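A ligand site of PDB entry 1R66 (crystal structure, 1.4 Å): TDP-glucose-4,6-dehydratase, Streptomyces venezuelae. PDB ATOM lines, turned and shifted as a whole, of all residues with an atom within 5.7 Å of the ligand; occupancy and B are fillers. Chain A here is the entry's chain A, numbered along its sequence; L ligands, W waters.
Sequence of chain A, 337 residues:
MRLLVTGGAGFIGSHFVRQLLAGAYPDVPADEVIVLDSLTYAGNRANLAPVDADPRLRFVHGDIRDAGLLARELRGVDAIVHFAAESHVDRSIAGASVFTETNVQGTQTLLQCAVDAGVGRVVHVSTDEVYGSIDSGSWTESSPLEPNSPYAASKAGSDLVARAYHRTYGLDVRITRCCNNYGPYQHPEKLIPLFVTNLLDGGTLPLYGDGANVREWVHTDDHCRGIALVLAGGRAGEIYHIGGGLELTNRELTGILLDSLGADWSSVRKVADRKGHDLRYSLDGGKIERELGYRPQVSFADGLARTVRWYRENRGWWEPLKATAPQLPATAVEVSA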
ATOM      1  N   SER A  87      -1.371  12.884  -0.682  1.00  0.00           N
ATOM      2  CA  SER A  87      -0.174  13.688  -0.395  1.00  0.00           C
ATOM      3  C   SER A  87       1.043  13.499  -1.293  1.00  0.00           C
ATOM      4  O   SER A  87       2.064  14.163  -1.036  1.00  0.00           O
ATOM      5  CB  SER A  87       0.235  13.391   1.054  1.00  0.00           C
ATOM      6  OG  SER A  87       0.842  12.100   1.094  1.00  0.00           O
ATOM      7  N   HIS A  88       0.950  12.643  -2.298  1.00  0.00           N
ATOM      8  CA  HIS A  88       2.156  12.455  -3.072  1.00  0.00           C
ATOM      9  C   HIS A  88       2.174  13.171  -4.436  1.00  0.00           C
ATOM     10  O   HIS A  88       1.310  12.923  -5.310  1.00  0.00           O
ATOM     11  CB  HIS A  88       2.442  10.953  -3.243  1.00  0.00           C
ATOM     12  CG  HIS A  88       3.894  10.729  -3.587  1.00  0.00           C
ATOM     13  ND1 HIS A  88       4.274   9.856  -4.582  1.00  0.00           N
ATOM     14  CD2 HIS A  88       5.035  11.296  -3.082  1.00  0.00           C
ATOM     15  CE1 HIS A  88       5.610   9.882  -4.632  1.00  0.00           C
ATOM     16  NE2 HIS A  88       6.113  10.739  -3.742  1.00  0.00           N
ATOM     17  N   VAL A  89       3.199  14.039  -4.638  1.00  0.00           N
ATOM     18  CA  VAL A  89       3.312  14.764  -5.894  1.00  0.00           C
ATOM     19  C   VAL A  89       3.292  13.895  -7.162  1.00  0.00           C
ATOM     20  O   VAL A  89       2.583  14.197  -8.133  1.00  0.00           O
ATOM     21  CB  VAL A  89       4.506  15.701  -5.855  1.00  0.00           C
ATOM     22  CG1 VAL A  89       4.630  16.361  -7.237  1.00  0.00           C
ATOM     23  CG2 VAL A  89       4.323  16.732  -4.736  1.00  0.00           C
ATOM     24  N   ASP A  90       4.080  12.800  -7.152  1.00  0.00           N
ATOM     25  CA  ASP A  90       4.110  11.899  -8.317  1.00  0.00           C
ATOM     26  C   ASP A  90       2.747  11.317  -8.670  1.00  0.00           C
ATOM     27  O   ASP A  90       2.397  11.161  -9.851  1.00  0.00           O
ATOM     28  CB  ASP A  90       5.261  10.836  -8.219  1.00  0.00           C
ATOM     29  CG  ASP A  90       6.638  11.472  -8.336  1.00  0.00           C
ATOM     30  OD1 ASP A  90       6.904  12.336  -9.141  1.00  0.00           O
ATOM     31  OD2 ASP A  90       7.523  11.060  -7.460  1.00  0.00           O
ATOM     32  N   GLU A 129       4.584  23.601  -0.377  1.00  0.00           N
ATOM     33  CA  GLU A 129       4.563  23.540  -1.843  1.00  0.00           C
ATOM     34  C   GLU A 129       3.590  24.529  -2.500  1.00  0.00           C
ATOM     35  O   GLU A 129       3.664  24.727  -3.731  1.00  0.00           O
ATOM     36  CB  GLU A 129       4.298  22.097  -2.287  1.00  0.00           C
ATOM     37  CG  GLU A 129       5.205  21.166  -1.430  1.00  0.00           C
ATOM     38  CD  GLU A 129       5.382  19.805  -2.005  1.00  0.00           C
ATOM     39  OE1 GLU A 129       4.951  19.466  -3.096  1.00  0.00           O
ATOM     40  OE2 GLU A 129       6.018  18.982  -1.192  1.00  0.00           O
ATOM     41  N   TYR A 151      -0.846  18.431  -6.990  1.00  0.00           N
ATOM     42  CA  TYR A 151      -0.943  18.245  -5.560  1.00  0.00           C
ATOM     43  C   TYR A 151      -0.893  19.630  -4.900  1.00  0.00           C
ATOM     44  O   TYR A 151      -1.733  19.974  -4.104  1.00  0.00           O
ATOM     45  CB  TYR A 151       0.207  17.351  -5.005  1.00  0.00           C
ATOM     46  CG  TYR A 151       0.423  17.521  -3.497  1.00  0.00           C
ATOM     47  CD1 TYR A 151      -0.518  17.059  -2.569  1.00  0.00           C
ATOM     48  CD2 TYR A 151       1.593  18.079  -3.005  1.00  0.00           C
ATOM     49  CE1 TYR A 151      -0.301  17.187  -1.203  1.00  0.00           C
ATOM     50  CE2 TYR A 151       1.818  18.253  -1.640  1.00  0.00           C
ATOM     51  CZ  TYR A 151       0.876  17.746  -0.742  1.00  0.00           C
ATOM     52  OH  TYR A 151       1.119  17.891   0.626  1.00  0.00           O
ATOM     53  N   ASN A 180       9.259  19.441   4.229  1.00  0.00           N
ATOM     54  CA  ASN A 180       9.236  17.982   4.188  1.00  0.00           C
ATOM     55  C   ASN A 180       9.481  17.382   5.531  1.00  0.00           C
ATOM     56  O   ASN A 180      10.395  17.761   6.235  1.00  0.00           O
ATOM     57  CB  ASN A 180      10.300  17.409   3.228  1.00  0.00           C
ATOM     58  CG  ASN A 180      10.019  17.769   1.795  1.00  0.00           C
ATOM     59  OD1 ASN A 180       9.886  18.955   1.429  1.00  0.00           O
ATOM     60  ND2 ASN A 180       9.944  16.757   0.950  1.00  0.00           N
ATOM     61  N   GLU A 189       6.906   5.344  -0.395  1.00  0.00           N
ATOM     62  CA  GLU A 189       6.935   5.979  -1.716  1.00  0.00           C
ATOM     63  C   GLU A 189       7.652   7.314  -1.627  1.00  0.00           C
ATOM     64  O   GLU A 189       8.030   7.920  -2.657  1.00  0.00           O
ATOM     65  CB  GLU A 189       5.498   6.230  -2.226  1.00  0.00           C
ATOM     66  CG  GLU A 189       4.712   7.274  -1.397  1.00  0.00           C
ATOM     67  CD  GLU A 189       3.311   7.521  -1.900  1.00  0.00           C
ATOM     68  OE1 GLU A 189       2.893   6.977  -2.913  1.00  0.00           O
ATOM     69  OE2 GLU A 189       2.596   8.326  -1.146  1.00  0.00           O
ATOM     70  N   LYS A 190       7.806   7.851  -0.396  1.00  0.00           N
ATOM     71  CA  LYS A 190       8.463   9.142  -0.139  1.00  0.00           C
ATOM     72  C   LYS A 190       9.983   8.956  -0.183  1.00  0.00           C
ATOM     73  O   LYS A 190      10.513   7.894   0.166  1.00  0.00           O
ATOM     74  CB  LYS A 190       8.024   9.817   1.165  1.00  0.00           C
ATOM     75  CG  LYS A 190       6.514  10.102   1.260  1.00  0.00           C
ATOM     76  CD  LYS A 190       5.895  10.942   0.111  1.00  0.00           C
ATOM     77  CE  LYS A 190       5.999  12.459   0.263  1.00  0.00           C
ATOM     78  NZ  LYS A 190       5.040  13.252  -0.528  1.00  0.00           N
ATOM     79  N   LEU A 191      10.692   9.998  -0.627  1.00  0.00           N
ATOM     80  CA  LEU A 191      12.152   9.922  -0.808  1.00  0.00           C
ATOM     81  C   LEU A 191      12.949   9.166   0.225  1.00  0.00           C
ATOM     82  O   LEU A 191      13.662   8.197  -0.082  1.00  0.00           O
ATOM     83  CB  LEU A 191      12.738  11.334  -0.941  1.00  0.00           C
ATOM     84  CG  LEU A 191      14.251  11.274  -1.163  1.00  0.00           C
ATOM     85  CD1 LEU A 191      14.505  10.738  -2.571  1.00  0.00           C
ATOM     86  CD2 LEU A 191      14.777  12.695  -1.137  1.00  0.00           C
ATOM     87  N   ILE A 192      12.947   9.643   1.473  1.00  0.00           N
ATOM     88  CA  ILE A 192      13.813   8.955   2.466  1.00  0.00           C
ATOM     89  C   ILE A 192      13.493   7.484   2.684  1.00  0.00           C
ATOM     90  O   ILE A 192      14.385   6.658   2.520  1.00  0.00           O
ATOM     91  CB  ILE A 192      13.897   9.770   3.750  1.00  0.00           C
ATOM     92  CG1 ILE A 192      14.628  11.087   3.496  1.00  0.00           C
ATOM     93  CG2 ILE A 192      14.450   9.013   4.950  1.00  0.00           C
ATOM     94  CD1 ILE A 192      14.584  12.047   4.684  1.00  0.00           C
ATOM     95  N   LEU A 194      11.863   5.561   0.813  1.00  0.00           N
ATOM     96  CA  LEU A 194      12.074   4.840  -0.437  1.00  0.00           C
ATOM     97  C   LEU A 194      13.531   4.507  -0.611  1.00  0.00           C
ATOM     98  O   LEU A 194      13.903   3.395  -0.990  1.00  0.00           O
ATOM     99  CB  LEU A 194      11.717   5.679  -1.672  1.00  0.00           C
ATOM    100  CG  LEU A 194      12.121   4.951  -2.955  1.00  0.00           C
ATOM    101  CD1 LEU A 194      11.213   3.737  -3.171  1.00  0.00           C
ATOM    102  CD2 LEU A 194      11.869   5.933  -4.084  1.00  0.00           C
ATOM    103  N   PHE A 195      14.407   5.469  -0.364  1.00  0.00           N
ATOM    104  CA  PHE A 195      15.786   5.177  -0.566  1.00  0.00           C
ATOM    105  C   PHE A 195      16.306   4.259   0.520  1.00  0.00           C
ATOM    106  O   PHE A 195      17.043   3.332   0.231  1.00  0.00           O
ATOM    107  CB  PHE A 195      16.557   6.498  -0.647  1.00  0.00           C
ATOM    108  CG  PHE A 195      16.530   7.171  -2.008  1.00  0.00           C
ATOM    109  CD1 PHE A 195      15.554   6.884  -2.966  1.00  0.00           C
ATOM    110  CD2 PHE A 195      17.529   8.105  -2.327  1.00  0.00           C
ATOM    111  CE1 PHE A 195      15.579   7.522  -4.204  1.00  0.00           C
ATOM    112  CE2 PHE A 195      17.549   8.782  -3.547  1.00  0.00           C
ATOM    113  CZ  PHE A 195      16.569   8.469  -4.489  1.00  0.00           C
ATOM    114  N   PRO A 206      16.591   5.765  -7.408  1.00  0.00           N
ATOM    115  CA  PRO A 206      16.202   6.597  -8.530  1.00  0.00           C
ATOM    116  C   PRO A 206      16.288   8.066  -8.234  1.00  0.00           C
ATOM    117  O   PRO A 206      15.336   8.656  -7.758  1.00  0.00           O
ATOM    118  CB  PRO A 206      14.736   6.225  -8.802  1.00  0.00           C
ATOM    119  CG  PRO A 206      14.196   5.617  -7.518  1.00  0.00           C
ATOM    120  CD  PRO A 206      15.427   5.149  -6.735  1.00  0.00           C
ATOM    121  N   LEU A 207      17.413   8.684  -8.505  1.00  0.00           N
ATOM    122  CA  LEU A 207      17.536  10.086  -8.215  1.00  0.00           C
ATOM    123  C   LEU A 207      17.100  10.941  -9.401  1.00  0.00           C
ATOM    124  O   LEU A 207      17.681  10.888 -10.469  1.00  0.00           O
ATOM    125  CB  LEU A 207      19.005  10.294  -7.824  1.00  0.00           C
ATOM    126  CG  LEU A 207      19.329  11.748  -7.493  1.00  0.00           C
ATOM    127  CD1 LEU A 207      18.619  12.191  -6.213  1.00  0.00           C
ATOM    128  CD2 LEU A 207      20.839  11.865  -7.298  1.00  0.00           C
ATOM    129  N   TYR A 208      16.061  11.744  -9.244  1.00  0.00           N
ATOM    130  CA  TYR A 208      15.559  12.513 -10.373  1.00  0.00           C
ATOM    131  C   TYR A 208      16.535  13.514 -10.912  1.00  0.00           C
ATOM    132  O   TYR A 208      17.165  14.237 -10.140  1.00  0.00           O
ATOM    133  CB  TYR A 208      14.292  13.306 -10.000  1.00  0.00           C
ATOM    134  CG  TYR A 208      13.093  12.447  -9.632  1.00  0.00           C
ATOM    135  CD1 TYR A 208      13.015  11.088  -9.926  1.00  0.00           C
ATOM    136  CD2 TYR A 208      12.033  13.037  -8.946  1.00  0.00           C
ATOM    137  CE1 TYR A 208      11.909  10.343  -9.530  1.00  0.00           C
ATOM    138  CE2 TYR A 208      10.910  12.317  -8.543  1.00  0.00           C
ATOM    139  CZ  TYR A 208      10.844  10.966  -8.866  1.00  0.00           C
ATOM    140  OH  TYR A 208       9.731  10.278  -8.468  1.00  0.00           O
ATOM    141  N   ASN A 213      17.772  19.609  -6.804  1.00  0.00           N
ATOM    142  CA  ASN A 213      16.623  20.177  -6.107  1.00  0.00           C
ATOM    143  C   ASN A 213      16.837  20.245  -4.599  1.00  0.00           C
ATOM    144  O   ASN A 213      17.460  19.354  -4.015  1.00  0.00           O
ATOM    145  CB  ASN A 213      15.332  19.429  -6.427  1.00  0.00           C
ATOM    146  CG  ASN A 213      15.211  19.243  -7.914  1.00  0.00           C
ATOM    147  OD1 ASN A 213      15.984  18.467  -8.501  1.00  0.00           O
ATOM    148  ND2 ASN A 213      14.249  19.933  -8.532  1.00  0.00           N
ATOM    149  N   ARG A 215      15.303  20.740  -0.609  1.00  0.00           N
ATOM    150  CA  ARG A 215      14.161  20.616   0.259  1.00  0.00           C
ATOM    151  C   ARG A 215      14.633  20.882   1.670  1.00  0.00           C
ATOM    152  O   ARG A 215      15.806  20.687   1.941  1.00  0.00           O
ATOM    153  CB  ARG A 215      13.524  19.215   0.182  1.00  0.00           C
ATOM    154  CG  ARG A 215      13.013  18.758  -1.206  1.00  0.00           C
ATOM    155  CD  ARG A 215      11.810  19.603  -1.604  1.00  0.00           C
ATOM    156  NE  ARG A 215      11.139  19.197  -2.850  1.00  0.00           N
ATOM    157  CZ  ARG A 215      11.439  19.821  -4.004  1.00  0.00           C
ATOM    158  NH1 ARG A 215      12.388  20.738  -4.140  1.00  0.00           N
ATOM    159  NH2 ARG A 215      10.787  19.478  -5.094  1.00  0.00           N
ATOM    160  N   TRP A 217      14.062  19.807   5.672  1.00  0.00           N
ATOM    161  CA  TRP A 217      13.562  18.623   6.341  1.00  0.00           C
ATOM    162  C   TRP A 217      13.363  18.848   7.802  1.00  0.00           C
ATOM    163  O   TRP A 217      14.268  19.351   8.502  1.00  0.00           O
ATOM    164  CB  TRP A 217      14.676  17.572   6.229  1.00  0.00           C
ATOM    165  CG  TRP A 217      14.854  17.179   4.794  1.00  0.00           C
ATOM    166  CD1 TRP A 217      15.729  17.716   3.886  1.00  0.00           C
ATOM    167  CD2 TRP A 217      14.012  16.283   4.058  1.00  0.00           C
ATOM    168  NE1 TRP A 217      15.520  17.161   2.644  1.00  0.00           N
ATOM    169  CE2 TRP A 217      14.465  16.276   2.710  1.00  0.00           C
ATOM    170  CE3 TRP A 217      12.916  15.458   4.427  1.00  0.00           C
ATOM    171  CZ2 TRP A 217      13.847  15.464   1.714  1.00  0.00           C
ATOM    172  CZ3 TRP A 217      12.295  14.672   3.446  1.00  0.00           C
ATOM    173  CH2 TRP A 217      12.754  14.670   2.109  1.00  0.00           C
ATOM    174  N   ASN A 250      18.946  17.113  -2.946  1.00  0.00           N
ATOM    175  CA  ASN A 250      18.644  15.691  -2.872  1.00  0.00           C
ATOM    176  C   ASN A 250      19.943  14.869  -2.997  1.00  0.00           C
ATOM    177  O   ASN A 250      20.056  13.773  -2.458  1.00  0.00           O
ATOM    178  CB  ASN A 250      17.679  15.334  -4.009  1.00  0.00           C
ATOM    179  CG  ASN A 250      16.317  15.952  -3.749  1.00  0.00           C
ATOM    180  OD1 ASN A 250      15.867  16.226  -2.621  1.00  0.00           O
ATOM    181  ND2 ASN A 250      15.615  16.166  -4.852  1.00  0.00           N
ATOM    182  N   ARG A 274      11.216  14.646 -12.756  1.00  0.00           N
ATOM    183  CA  ARG A 274       9.775  14.815 -12.526  1.00  0.00           C
ATOM    184  C   ARG A 274       9.245  16.050 -13.299  1.00  0.00           C
ATOM    185  O   ARG A 274       9.884  17.140 -13.298  1.00  0.00           O
ATOM    186  CB  ARG A 274       9.589  15.061 -11.019  1.00  0.00           C
ATOM    187  CG  ARG A 274       8.174  15.507 -10.640  1.00  0.00           C
ATOM    188  CD  ARG A 274       8.207  15.825  -9.141  1.00  0.00           C
ATOM    189  NE  ARG A 274       8.204  14.651  -8.274  1.00  0.00           N
ATOM    190  CZ  ARG A 274       8.310  14.800  -6.968  1.00  0.00           C
ATOM    191  NH1 ARG A 274       8.449  16.019  -6.431  1.00  0.00           N
ATOM    192  NH2 ARG A 274       8.227  13.728  -6.177  1.00  0.00           N
ATOM    193  N   HIS A 277       9.039  19.692 -11.870  1.00  0.00           N
ATOM    194  CA  HIS A 277       9.757  19.554 -10.609  1.00  0.00           C
ATOM    195  C   HIS A 277      10.159  20.866  -9.955  1.00  0.00           C
ATOM    196  O   HIS A 277      10.889  21.659 -10.545  1.00  0.00           O
ATOM    197  CB  HIS A 277      10.989  18.673 -10.835  1.00  0.00           C
ATOM    198  CG  HIS A 277      11.544  18.084  -9.568  1.00  0.00           C
ATOM    199  ND1 HIS A 277      12.670  17.242  -9.596  1.00  0.00           N
ATOM    200  CD2 HIS A 277      11.195  18.222  -8.260  1.00  0.00           C
ATOM    201  CE1 HIS A 277      12.957  16.908  -8.342  1.00  0.00           C
ATOM    202  NE2 HIS A 277      12.089  17.475  -7.517  1.00  0.00           N
ATOM    203  N   ASP A 278       9.731  21.104  -8.713  1.00  0.00           N
ATOM    204  CA  ASP A 278      10.100  22.345  -8.021  1.00  0.00           C
ATOM    205  C   ASP A 278      11.561  22.330  -7.646  1.00  0.00           C
ATOM    206  O   ASP A 278      12.097  21.407  -6.992  1.00  0.00           O
ATOM    207  CB  ASP A 278       9.251  22.592  -6.753  1.00  0.00           C
ATOM    208  CG  ASP A 278       7.815  22.928  -7.081  1.00  0.00           C
ATOM    209  OD1 ASP A 278       7.534  23.560  -8.058  1.00  0.00           O
ATOM    210  OD2 ASP A 278       6.912  22.481  -6.265  1.00  0.00           O
ATOM    211  N   TYR A 281      12.526  24.645  -1.999  1.00  0.00           N
ATOM    212  CA  TYR A 281      11.574  25.080  -0.983  1.00  0.00           C
ATOM    213  C   TYR A 281      12.373  25.583   0.225  1.00  0.00           C
ATOM    214  O   TYR A 281      13.389  24.969   0.590  1.00  0.00           O
ATOM    215  CB  TYR A 281      10.626  23.965  -0.439  1.00  0.00           C
ATOM    216  CG  TYR A 281       9.753  23.245  -1.463  1.00  0.00           C
ATOM    217  CD1 TYR A 281       9.253  23.885  -2.599  1.00  0.00           C
ATOM    218  CD2 TYR A 281       9.438  21.904  -1.268  1.00  0.00           C
ATOM    219  CE1 TYR A 281       8.430  23.239  -3.529  1.00  0.00           C
ATOM    220  CE2 TYR A 281       8.633  21.229  -2.195  1.00  0.00           C
ATOM    221  CZ  TYR A 281       8.130  21.895  -3.315  1.00  0.00           C
ATOM    222  OH  TYR A 281       7.340  21.228  -4.200  1.00  0.00           O
HETATM  223  P1  LIG L   1       9.033  13.496  -2.372  1.00  0.00           P
HETATM  224  O1  LIG L   1       9.338  12.537  -1.251  1.00  0.00           O
HETATM  225  O2  LIG L   1       8.115  12.958  -3.416  1.00  0.00           O
HETATM  226  O3  LIG L   1       8.380  14.808  -1.698  1.00  0.00           O
HETATM  227  P2  LIG L   1       8.029  16.256  -2.283  1.00  0.00           P
HETATM  228  O4  LIG L   1       9.144  17.370  -1.997  1.00  0.00           O
HETATM  229  O5  LIG L   1       6.752  16.646  -1.605  1.00  0.00           O
HETATM  230  O6  LIG L   1       7.838  16.117  -3.786  1.00  0.00           O
HETATM  231  O7  LIG L   1      10.357  14.012  -3.136  1.00  0.00           O
HETATM  232  C1  LIG L   1      11.333  14.704  -2.359  1.00  0.00           C
HETATM  233  C2  LIG L   1      12.382  15.140  -3.340  1.00  0.00           C
HETATM  234  O8  LIG L   1      13.046  13.919  -3.759  1.00  0.00           O
HETATM  235  C3  LIG L   1      11.836  15.834  -4.585  1.00  0.00           C
HETATM  236  O9  LIG L   1      12.750  16.837  -5.069  1.00  0.00           O
HETATM  237  C4  LIG L   1      11.716  14.647  -5.556  1.00  0.00           C
HETATM  238  C5  LIG L   1      12.934  13.792  -5.172  1.00  0.00           C
HETATM  239  N1  LIG L   1      12.802  12.349  -5.480  1.00  0.00           N
HETATM  240  C6  LIG L   1      13.765  11.673  -6.190  1.00  0.00           C
HETATM  241  O10 LIG L   1      14.793  12.178  -6.633  1.00  0.00           O
HETATM  242  N2  LIG L   1      13.495  10.341  -6.344  1.00  0.00           N
HETATM  243  C7  LIG L   1      12.385   9.650  -5.865  1.00  0.00           C
HETATM  244  O11 LIG L   1      12.278   8.464  -6.130  1.00  0.00           O
HETATM  245  C8  LIG L   1      11.437  10.428  -5.144  1.00  0.00           C
HETATM  246  C9  LIG L   1      10.157   9.805  -4.569  1.00  0.00           C
HETATM  247  C10 LIG L   1      11.686  11.709  -4.969  1.00  0.00           C
HETATM  248  O   HOH W   1      10.190   6.900  -7.264  1.00  0.00           O
HETATM  249  O   HOH W   2       7.957  18.605  -4.965  1.00  0.00           O
HETATM  250  O   HOH W   3       5.676  14.145  -2.893  1.00  0.00           O
HETATM  251  O   HOH W   4       9.651  13.568   1.437  1.00  0.00           O
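OE2 of Glu 129 lies close to O5 of the ligand (2.5 Å).
A ring nitrogen (NE2) of His 277 sits at hydrogen-bond distance from an oxygen (O9) of the ligand, at 2.6 Å.
The guanidinium group (NH1) of Arg 274 lies within salt-bridge range of an oxygen (O6) of the ligand (2.7 Å).
The guanidinium group (NE) of Arg 215 lies within salt-bridge range of an oxygen (O4) of the ligand, 2.8 Å away.
N2 of the ligand sits at hydrogen-bond distance from O of Pro 206 (2.9 Å).
The backbone NH (N) of Tyr 208 is in hydrogen-bond range of an oxygen (O10) of the ligand (2.9 Å).
N of Leu 191 lies within hydrogen-bond range of O1 of the ligand (2.9 Å).
An oxygen (O9) of the ligand sits at hydrogen-bond distance from the side-chain amide nitrogen (ND2) of Asn 250, at 3.0 Å.
An oxygen (O2) of the ligand is in hydrogen-bond range of a ring nitrogen (NE2) of His 88 (3.0 Å).
The side-chain amide nitrogen (ND2) of Asn 180 lies within hydrogen-bond range of an oxygen (O4) of the ligand.
O5 of the ligand lies within salt-bridge range of NZ of Lys 190 (3.95 Å).
Merely in contact with the ligand: Leu 194 (3.3 Å), Glu 189 (3.4 Å), Val 89 (3.7 Å), Leu 207 (3.8 Å), Tyr 281 (3.9 Å), Asn 213 (3.9 Å) and Phe 195 (3.9 Å).
Hydrophobic or aromatic side chains that line the ligand: His 88, Val 89, Leu 191, Leu 194, Phe 195, Pro 206, Leu 207, Tyr 208, His 277 and Tyr 281.
Within 4 Å of the ligand: His 88, Val 89, Glu 129, Asn 180, Glu 189, Lys 190, Leu 191, Leu 194, Phe 195, Pro 206, Leu 207, Tyr 208, Asn 213, Arg 215, Asn 250, Arg 274, His 277 and Tyr 281.
The nearest printed residue that does not touch the ligand is Asp 90 (4.1 Å).
OH of Tyr 281 lies within hydrogen-bond range of OE1 of Glu 129 (3.2 Å).
The guanidinium group of Arg 215 sits at hydrogen-bond distance from a ring nitrogen (NE2) of His 277 (3.4 Å).
A ring nitrogen (ND1) of His 277 lies close to the side-chain amide nitrogen (ND2) of Asn 213 (3.3 Å).
The guanidinium group of Arg 274 is in salt-bridge range of the side-chain carboxylate of Asp 90 (2.8 Å).
O of Asp 278 is in hydrogen-bond range of NH1 of Arg 215.
O of Asn 213 is in hydrogen-bond range of N of Asn 250 (2.9 Å).
The side-chain hydroxyl of Tyr 281 is in hydrogen-bond range of the side-chain carboxylate of Asp 278, 2.5 Å away.
O of Asp 278 sits at hydrogen-bond distance from ND2 of Asn 213 (3.0 Å).
Water W2 lies within hydrogen-bond range of an oxygen (O6) of the ligand (2.8 Å), the side-chain hydroxyl of Tyr 281 (2.8 Å), the guanidinium group of Arg 215 (3.0 Å) and the guanidinium group of Arg 274 (3.0 Å).
Water W3 lies within hydrogen-bond range of the side-chain amino group of Lys 190 (2.6 Å), an oxygen (O2) of the ligand (2.8 Å) and the backbone NH of Val 89 (3.0 Å).
Water W4 lies within hydrogen-bond range of O1 of the ligand (2.9 Å) and ND2 of Asn 180 (3.2 Å).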
